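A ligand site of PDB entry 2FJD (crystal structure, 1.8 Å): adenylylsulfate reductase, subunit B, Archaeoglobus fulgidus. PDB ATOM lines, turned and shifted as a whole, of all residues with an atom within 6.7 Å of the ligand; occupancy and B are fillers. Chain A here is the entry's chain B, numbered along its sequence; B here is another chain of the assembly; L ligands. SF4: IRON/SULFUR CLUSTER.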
ATOM      1  N   PRO A   2      10.648 -10.715   9.995  1.00  0.00           N
ATOM      2  CA  PRO A   2      11.068 -10.383   8.637  1.00  0.00           C
ATOM      3  C   PRO A   2      12.465  -9.769   8.599  1.00  0.00           C
ATOM      4  O   PRO A   2      12.962  -9.258   9.601  1.00  0.00           O
ATOM      5  CB  PRO A   2       9.991  -9.405   8.171  1.00  0.00           C
ATOM      6  CG  PRO A   2       8.767  -9.927   8.879  1.00  0.00           C
ATOM      7  CD  PRO A   2       9.292 -10.214  10.270  1.00  0.00           C
ATOM      8  N   SER A   3      13.094  -9.820   7.428  1.00  0.00           N
ATOM      9  CA  SER A   3      14.442  -9.266   7.278  1.00  0.00           C
ATOM     10  C   SER A   3      14.393  -7.750   7.215  1.00  0.00           C
ATOM     11  O   SER A   3      13.371  -7.156   6.855  1.00  0.00           O
ATOM     12  CB  SER A   3      15.094  -9.794   5.992  1.00  0.00           C
ATOM     13  OG  SER A   3      14.437  -9.266   4.849  1.00  0.00           O
ATOM     14  N   CYS A  21      21.429  -9.746  -1.809  1.00  0.00           N
ATOM     15  CA  CYS A  21      20.101  -9.921  -1.234  1.00  0.00           C
ATOM     16  C   CYS A  21      18.998  -9.961  -2.301  1.00  0.00           C
ATOM     17  O   CYS A  21      18.114 -10.810  -2.258  1.00  0.00           O
ATOM     18  CB  CYS A  21      19.818  -8.820  -0.217  1.00  0.00           C
ATOM     19  SG  CYS A  21      19.835  -7.134  -0.870  1.00  0.00           S
ATOM     20  N   ILE A  24      19.264 -13.360  -4.270  1.00  0.00           N
ATOM     21  CA  ILE A  24      18.911 -14.604  -3.589  1.00  0.00           C
ATOM     22  C   ILE A  24      17.485 -14.835  -3.082  1.00  0.00           C
ATOM     23  O   ILE A  24      17.017 -15.966  -3.066  1.00  0.00           O
ATOM     24  CB  ILE A  24      19.883 -14.832  -2.401  1.00  0.00           C
ATOM     25  CG1 ILE A  24      19.991 -16.331  -2.086  1.00  0.00           C
ATOM     26  CG2 ILE A  24      19.414 -14.061  -1.178  1.00  0.00           C
ATOM     27  CD1 ILE A  24      20.746 -17.122  -3.139  1.00  0.00           C
ATOM     28  N   CYS A  25      16.790 -13.765  -2.668  1.00  0.00           N
ATOM     29  CA  CYS A  25      15.440 -13.908  -2.107  1.00  0.00           C
ATOM     30  C   CYS A  25      14.456 -14.729  -2.928  1.00  0.00           C
ATOM     31  O   CYS A  25      14.066 -14.350  -4.032  1.00  0.00           O
ATOM     32  CB  CYS A  25      14.824 -12.533  -1.854  1.00  0.00           C
ATOM     33  SG  CYS A  25      13.197 -12.653  -1.059  1.00  0.00           S
ATOM     34  N   PRO A  26      14.020 -15.877  -2.380  1.00  0.00           N
ATOM     35  CA  PRO A  26      13.077 -16.797  -3.032  1.00  0.00           C
ATOM     36  C   PRO A  26      11.687 -16.202  -3.273  1.00  0.00           C
ATOM     37  O   PRO A  26      10.904 -16.768  -4.047  1.00  0.00           O
ATOM     38  CB  PRO A  26      13.029 -17.984  -2.073  1.00  0.00           C
ATOM     39  CG  PRO A  26      14.345 -17.918  -1.343  1.00  0.00           C
ATOM     40  CD  PRO A  26      14.494 -16.445  -1.099  1.00  0.00           C
ATOM     41  N   ASN A  27      11.366 -15.097  -2.609  1.00  0.00           N
ATOM     42  CA  ASN A  27      10.055 -14.487  -2.784  1.00  0.00           C
ATOM     43  C   ASN A  27      10.125 -13.083  -3.386  1.00  0.00           C
ATOM     44  O   ASN A  27       9.139 -12.355  -3.361  1.00  0.00           O
ATOM     45  CB  ASN A  27       9.298 -14.455  -1.444  1.00  0.00           C
ATOM     46  CG  ASN A  27       7.809 -14.738  -1.622  1.00  0.00           C
ATOM     47  OD1 ASN A  27       7.382 -15.270  -2.651  1.00  0.00           O
ATOM     48  ND2 ASN A  27       7.020 -14.398  -0.609  1.00  0.00           N
ATOM     49  N   ASP A  28      11.286 -12.712  -3.922  1.00  0.00           N
ATOM     50  CA  ASP A  28      11.484 -11.409  -4.560  1.00  0.00           C
ATOM     51  C   ASP A  28      11.162 -10.209  -3.666  1.00  0.00           C
ATOM     52  O   ASP A  28      10.544  -9.228  -4.119  1.00  0.00           O
ATOM     53  CB  ASP A  28      10.648 -11.343  -5.854  1.00  0.00           C
ATOM     54  CG  ASP A  28      10.916 -10.082  -6.668  1.00  0.00           C
ATOM     55  OD1 ASP A  28      12.101  -9.739  -6.837  1.00  0.00           O
ATOM     56  OD2 ASP A  28       9.945  -9.447  -7.129  1.00  0.00           O
ATOM     57  N   LEU A  29      11.608 -10.262  -2.416  1.00  0.00           N
ATOM     58  CA  LEU A  29      11.345  -9.180  -1.477  1.00  0.00           C
ATOM     59  C   LEU A  29      12.452  -8.137  -1.369  1.00  0.00           C
ATOM     60  O   LEU A  29      12.172  -6.956  -1.171  1.00  0.00           O
ATOM     61  CB  LEU A  29      11.089  -9.755  -0.082  1.00  0.00           C
ATOM     62  CG  LEU A  29      10.053 -10.878   0.026  1.00  0.00           C
ATOM     63  CD1 LEU A  29       9.867 -11.231   1.493  1.00  0.00           C
ATOM     64  CD2 LEU A  29       8.728 -10.442  -0.602  1.00  0.00           C
ATOM     65  N   MET A  30      13.696  -8.570  -1.489  1.00  0.00           N
ATOM     66  CA  MET A  30      14.828  -7.643  -1.373  1.00  0.00           C
ATOM     67  C   MET A  30      15.057  -6.854  -2.656  1.00  0.00           C
ATOM     68  O   MET A  30      15.108  -7.415  -3.752  1.00  0.00           O
ATOM     69  CB  MET A  30      16.096  -8.416  -1.003  1.00  0.00           C
ATOM     70  CG  MET A  30      16.009  -9.169   0.320  1.00  0.00           C
ATOM     71  SD  MET A  30      15.398  -8.154   1.691  1.00  0.00           S
ATOM     72  CE  MET A  30      16.747  -7.002   1.892  1.00  0.00           C
ATOM     73  N   ASN A  41      13.452  -4.602   2.448  1.00  0.00           N
ATOM     74  CA  ASN A  41      12.478  -5.658   2.191  1.00  0.00           C
ATOM     75  C   ASN A  41      11.225  -4.911   1.748  1.00  0.00           C
ATOM     76  O   ASN A  41      10.667  -4.106   2.496  1.00  0.00           O
ATOM     77  CB  ASN A  41      12.199  -6.433   3.490  1.00  0.00           C
ATOM     78  CG  ASN A  41      11.247  -7.597   3.276  1.00  0.00           C
ATOM     79  OD1 ASN A  41      10.227  -7.458   2.610  1.00  0.00           O
ATOM     80  ND2 ASN A  41      11.580  -8.746   3.853  1.00  0.00           N
ATOM     81  N   PRO A  44       7.415  -7.164   3.721  1.00  0.00           N
ATOM     82  CA  PRO A  44       7.703  -7.987   4.904  1.00  0.00           C
ATOM     83  C   PRO A  44       6.680  -9.034   5.316  1.00  0.00           C
ATOM     84  O   PRO A  44       7.049 -10.051   5.910  1.00  0.00           O
ATOM     85  CB  PRO A  44       7.961  -6.954   5.993  1.00  0.00           C
ATOM     86  CG  PRO A  44       7.130  -5.794   5.567  1.00  0.00           C
ATOM     87  CD  PRO A  44       7.373  -5.741   4.078  1.00  0.00           C
ATOM     88  N   MET A  46       5.349 -11.029   3.519  1.00  0.00           N
ATOM     89  CA  MET A  46       5.520 -12.135   2.575  1.00  0.00           C
ATOM     90  C   MET A  46       6.892 -12.769   2.797  1.00  0.00           C
ATOM     91  O   MET A  46       7.336 -13.604   2.007  1.00  0.00           O
ATOM     92  CB  MET A  46       5.397 -11.647   1.133  1.00  0.00           C
ATOM     93  CG  MET A  46       3.963 -11.409   0.661  1.00  0.00           C
ATOM     94  SD  MET A  46       2.977 -12.932   0.702  1.00  0.00           S
ATOM     95  CE  MET A  46       3.637 -13.831  -0.690  1.00  0.00           C
ATOM     96  N   CYS A  47       7.559 -12.350   3.875  1.00  0.00           N
ATOM     97  CA  CYS A  47       8.885 -12.865   4.228  1.00  0.00           C
ATOM     98  C   CYS A  47       8.747 -14.172   5.015  1.00  0.00           C
ATOM     99  O   CYS A  47       8.029 -14.228   6.017  1.00  0.00           O
ATOM    100  CB  CYS A  47       9.651 -11.837   5.074  1.00  0.00           C
ATOM    101  SG  CYS A  47      11.315 -12.318   5.611  1.00  0.00           S
ATOM    102  N   TRP A  48       9.439 -15.207   4.566  1.00  0.00           N
ATOM    103  CA  TRP A  48       9.389 -16.530   5.194  1.00  0.00           C
ATOM    104  C   TRP A  48      10.429 -16.665   6.301  1.00  0.00           C
ATOM    105  O   TRP A  48      10.466 -17.676   7.016  1.00  0.00           O
ATOM    106  CB  TRP A  48       9.632 -17.599   4.120  1.00  0.00           C
ATOM    107  CG  TRP A  48       9.025 -18.963   4.401  1.00  0.00           C
ATOM    108  CD1 TRP A  48       7.750 -19.207   4.847  1.00  0.00           C
ATOM    109  CD2 TRP A  48       9.629 -20.241   4.166  1.00  0.00           C
ATOM    110  NE1 TRP A  48       7.523 -20.564   4.901  1.00  0.00           N
ATOM    111  CE2 TRP A  48       8.661 -21.227   4.493  1.00  0.00           C
ATOM    112  CE3 TRP A  48      10.889 -20.653   3.711  1.00  0.00           C
ATOM    113  CZ2 TRP A  48       8.908 -22.590   4.377  1.00  0.00           C
ATOM    114  CZ3 TRP A  48      11.139 -22.025   3.605  1.00  0.00           C
ATOM    115  CH2 TRP A  48      10.152 -22.974   3.930  1.00  0.00           C
ATOM    116  N   GLU A  49      11.253 -15.630   6.468  1.00  0.00           N
ATOM    117  CA  GLU A  49      12.336 -15.617   7.441  1.00  0.00           C
ATOM    118  C   GLU A  49      13.242 -16.822   7.188  1.00  0.00           C
ATOM    119  O   GLU A  49      13.594 -17.565   8.101  1.00  0.00           O
ATOM    120  CB  GLU A  49      11.813 -15.621   8.887  1.00  0.00           C
ATOM    121  CG  GLU A  49      11.178 -14.292   9.314  1.00  0.00           C
ATOM    122  CD  GLU A  49      10.991 -14.144  10.825  1.00  0.00           C
ATOM    123  OE1 GLU A  49      11.080 -15.153  11.556  1.00  0.00           O
ATOM    124  OE2 GLU A  49      10.735 -13.012  11.287  1.00  0.00           O
ATOM    125  N   CYS A  50      13.602 -17.008   5.919  1.00  0.00           N
ATOM    126  CA  CYS A  50      14.455 -18.122   5.511  1.00  0.00           C
ATOM    127  C   CYS A  50      15.936 -17.802   5.723  1.00  0.00           C
ATOM    128  O   CYS A  50      16.781 -18.690   5.628  1.00  0.00           O
ATOM    129  CB  CYS A  50      14.203 -18.477   4.047  1.00  0.00           C
ATOM    130  SG  CYS A  50      14.902 -17.320   2.824  1.00  0.00           S
ATOM    131  N   TYR A  51      16.236 -16.524   5.979  1.00  0.00           N
ATOM    132  CA  TYR A  51      17.593 -16.057   6.215  1.00  0.00           C
ATOM    133  C   TYR A  51      18.556 -16.153   5.040  1.00  0.00           C
ATOM    134  O   TYR A  51      19.771 -16.004   5.207  1.00  0.00           O
ATOM    135  CB  TYR A  51      18.219 -16.765   7.423  1.00  0.00           C
ATOM    136  CG  TYR A  51      17.773 -16.220   8.762  1.00  0.00           C
ATOM    137  CD1 TYR A  51      16.475 -16.423   9.231  1.00  0.00           C
ATOM    138  CD2 TYR A  51      18.656 -15.513   9.571  1.00  0.00           C
ATOM    139  CE1 TYR A  51      16.066 -15.921  10.466  1.00  0.00           C
ATOM    140  CE2 TYR A  51      18.260 -15.006  10.808  1.00  0.00           C
ATOM    141  CZ  TYR A  51      16.960 -15.211  11.247  1.00  0.00           C
ATOM    142  OH  TYR A  51      16.567 -14.724  12.476  1.00  0.00           O
ATOM    143  N   SER A  52      18.031 -16.389   3.842  1.00  0.00           N
ATOM    144  CA  SER A  52      18.899 -16.488   2.671  1.00  0.00           C
ATOM    145  C   SER A  52      19.625 -15.164   2.428  1.00  0.00           C
ATOM    146  O   SER A  52      20.835 -15.141   2.190  1.00  0.00           O
ATOM    147  CB  SER A  52      18.085 -16.882   1.428  1.00  0.00           C
ATOM    148  OG  SER A  52      17.610 -18.219   1.535  1.00  0.00           O
ATOM    149  N   CYS A  53      18.881 -14.068   2.490  1.00  0.00           N
ATOM    150  CA  CYS A  53      19.460 -12.750   2.283  1.00  0.00           C
ATOM    151  C   CYS A  53      20.513 -12.464   3.353  1.00  0.00           C
ATOM    152  O   CYS A  53      21.619 -12.017   3.046  1.00  0.00           O
ATOM    153  CB  CYS A  53      18.373 -11.675   2.316  1.00  0.00           C
ATOM    154  SG  CYS A  53      17.398 -11.660   3.841  1.00  0.00           S
ATOM    155  N   VAL A  54      20.173 -12.749   4.607  1.00  0.00           N
ATOM    156  CA  VAL A  54      21.083 -12.528   5.727  1.00  0.00           C
ATOM    157  C   VAL A  54      22.419 -13.231   5.515  1.00  0.00           C
ATOM    158  O   VAL A  54      23.484 -12.628   5.661  1.00  0.00           O
ATOM    159  CB  VAL A  54      20.483 -13.059   7.043  1.00  0.00           C
ATOM    160  CG1 VAL A  54      21.512 -12.952   8.167  1.00  0.00           C
ATOM    161  CG2 VAL A  54      19.233 -12.266   7.392  1.00  0.00           C
ATOM    162  N   ILE A  62      22.290  -7.372   6.929  1.00  0.00           N
ATOM    163  CA  ILE A  62      20.906  -7.824   7.033  1.00  0.00           C
ATOM    164  C   ILE A  62      20.691  -8.681   8.284  1.00  0.00           C
ATOM    165  O   ILE A  62      21.502  -9.531   8.608  1.00  0.00           O
ATOM    166  CB  ILE A  62      20.488  -8.633   5.789  1.00  0.00           C
ATOM    167  CG1 ILE A  62      20.779  -7.815   4.532  1.00  0.00           C
ATOM    168  CG2 ILE A  62      19.004  -8.966   5.850  1.00  0.00           C
ATOM    169  CD1 ILE A  62      20.412  -8.519   3.248  1.00  0.00           C
ATOM    170  N   VAL A  64      17.226 -10.223  11.025  1.00  0.00           N
ATOM    171  CA  VAL A  64      15.825 -10.557  11.016  1.00  0.00           C
ATOM    172  C   VAL A  64      15.224 -10.198  12.362  1.00  0.00           C
ATOM    173  O   VAL A  64      15.791 -10.485  13.411  1.00  0.00           O
ATOM    174  CB  VAL A  64      15.607 -12.058  10.739  1.00  0.00           C
ATOM    175  CG1 VAL A  64      14.154 -12.440  11.023  1.00  0.00           C
ATOM    176  CG2 VAL A  64      15.940 -12.358   9.286  1.00  0.00           C
ATOM    177  N   ALA B  67      14.744 -23.576   0.862  1.00  0.00           N
ATOM    178  CA  ALA B  67      15.498 -22.323   0.985  1.00  0.00           C
ATOM    179  C   ALA B  67      16.371 -22.227   2.236  1.00  0.00           C
ATOM    180  O   ALA B  67      17.520 -21.786   2.148  1.00  0.00           O
ATOM    181  CB  ALA B  67      14.538 -21.141   0.933  1.00  0.00           C
ATOM    182  N   ILE B 237       6.028 -20.598   1.306  1.00  0.00           N
ATOM    183  CA  ILE B 237       5.189 -19.465   0.916  1.00  0.00           C
ATOM    184  C   ILE B 237       5.465 -19.116  -0.551  1.00  0.00           C
ATOM    185  O   ILE B 237       4.656 -18.460  -1.207  1.00  0.00           O
ATOM    186  CB  ILE B 237       5.492 -18.241   1.815  1.00  0.00           C
ATOM    187  CG1 ILE B 237       4.477 -17.124   1.544  1.00  0.00           C
ATOM    188  CG2 ILE B 237       6.910 -17.745   1.550  1.00  0.00           C
ATOM    189  CD1 ILE B 237       4.613 -15.949   2.492  1.00  0.00           C
ATOM    190  N   PHE B 238       6.605 -19.580  -1.046  1.00  0.00           N
ATOM    191  CA  PHE B 238       7.017 -19.323  -2.429  1.00  0.00           C
ATOM    192  C   PHE B 238       6.205 -20.108  -3.454  1.00  0.00           C
ATOM    193  O   PHE B 238       6.159 -19.742  -4.632  1.00  0.00           O
ATOM    194  CB  PHE B 238       8.501 -19.672  -2.618  1.00  0.00           C
ATOM    195  CG  PHE B 238       9.372 -19.291  -1.449  1.00  0.00           C
ATOM    196  CD1 PHE B 238      10.108 -20.267  -0.786  1.00  0.00           C
ATOM    197  CD2 PHE B 238       9.445 -17.978  -1.017  1.00  0.00           C
ATOM    198  CE1 PHE B 238      10.917 -19.926   0.291  1.00  0.00           C
ATOM    199  CE2 PHE B 238      10.251 -17.631   0.066  1.00  0.00           C
ATOM    200  CZ  PHE B 238      10.986 -18.606   0.729  1.00  0.00           C
HETATM  201 FE1  SF4 L   1      13.573 -13.142   1.256  1.00  0.00          FE
HETATM  202 FE2  SF4 L   1      12.695 -12.945   3.822  1.00  0.00          FE
HETATM  203 FE3  SF4 L   1      14.159 -15.049   2.976  1.00  0.00          FE
HETATM  204 FE4  SF4 L   1      15.312 -12.633   3.177  1.00  0.00          FE
HETATM  205  S1  SF4 L   1      14.428 -13.881   4.929  1.00  0.00           S
HETATM  206  S2  SF4 L   1      15.612 -14.078   1.585  1.00  0.00           S
HETATM  207  S3  SF4 L   1      13.593 -11.291   2.605  1.00  0.00           S
HETATM  208  S4  SF4 L   1      12.049 -14.511   2.362  1.00  0.00           S
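The side-chain sulfur (SG) of Cys 25 is bound to an iron atom (FE1) of the ligand, at 2.4 Å. SG of Cys 53 is bound to FE4 of the ligand, at 2.4 Å. OG of Ser 3 lies close to S3 of the ligand (3.1 Å). An iron atom (FE2) of the ligand is bound by the side-chain sulfur (SG) of Cys 47 (2.3 Å). A sulfur (S4) of the ligand lies close to the backbone NH (N) of Trp 48. A sulfur (S2) of the ligand lies close to the backbone NH (N) of Cys 53 (3.4 Å). The side-chain amide nitrogen (ND2) of Asn 41 sits close to a sulfur (S3) of the ligand (3.5 Å). The side-chain sulfur (SG) of Cys 50 is bound to an iron atom (FE3) of the ligand (2.4 Å). N of Tyr 51 lies close to S1 of the ligand (3.4 Å). The backbone NH of Cys 50 sits close to a sulfur (S1) of the ligand (3.4 Å).
The side-chain sulfur (SG) of Cys 50 lies close to the side-chain hydroxyl (OG) of Ser 52 (3.1 Å). The side-chain sulfur (SD) of Met 30 lies within hydrogen-bond range of the side-chain hydroxyl (OG) of Ser 3, at 3.5 Å. The side-chain sulfur of Cys 25 sits close to the backbone NH of Asp 28. SG of Cys 47 lies close to N of Glu 49, at 3.4 Å. N of Leu 29 sits close to SG of Cys 25. The side-chain hydroxyl (OG) of Ser 3 sits at hydrogen-bond distance from the side-chain amide nitrogen (ND2) of Asn 41 (3.1 Å). N of Asn 27 sits close to SG of Cys 25 (3.4 Å). The side-chain carboxylate (OE2) of Glu 49 lies close to the backbone nitrogen (N) of Pro 2, at 2.6 Å.
A sulfur (S3) of the ligand sits close to the side-chain sulfur of Met 30, at 3.7 Å. Pro 26 touches the ligand. Leu 29 touches the ligand. CA of Glu 49 touches S1 of the ligand, at 3.7 Å. Ser 52 touches the ligand. Hydrophobic or aromatic side chains that line the ligand: Pro 26, Leu 29 and Met 30. 13 residues have an atom within 4 Å of the ligand: Ser 3, Cys 25, Pro 26, Leu 29, Met 30, Asn 41, Cys 47, Trp 48, Glu 49, Cys 50, Tyr 51, Ser 52 and Cys 53. The nearest printed residue that does not touch the ligand is Phe 238 of chain B (4.3 Å).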
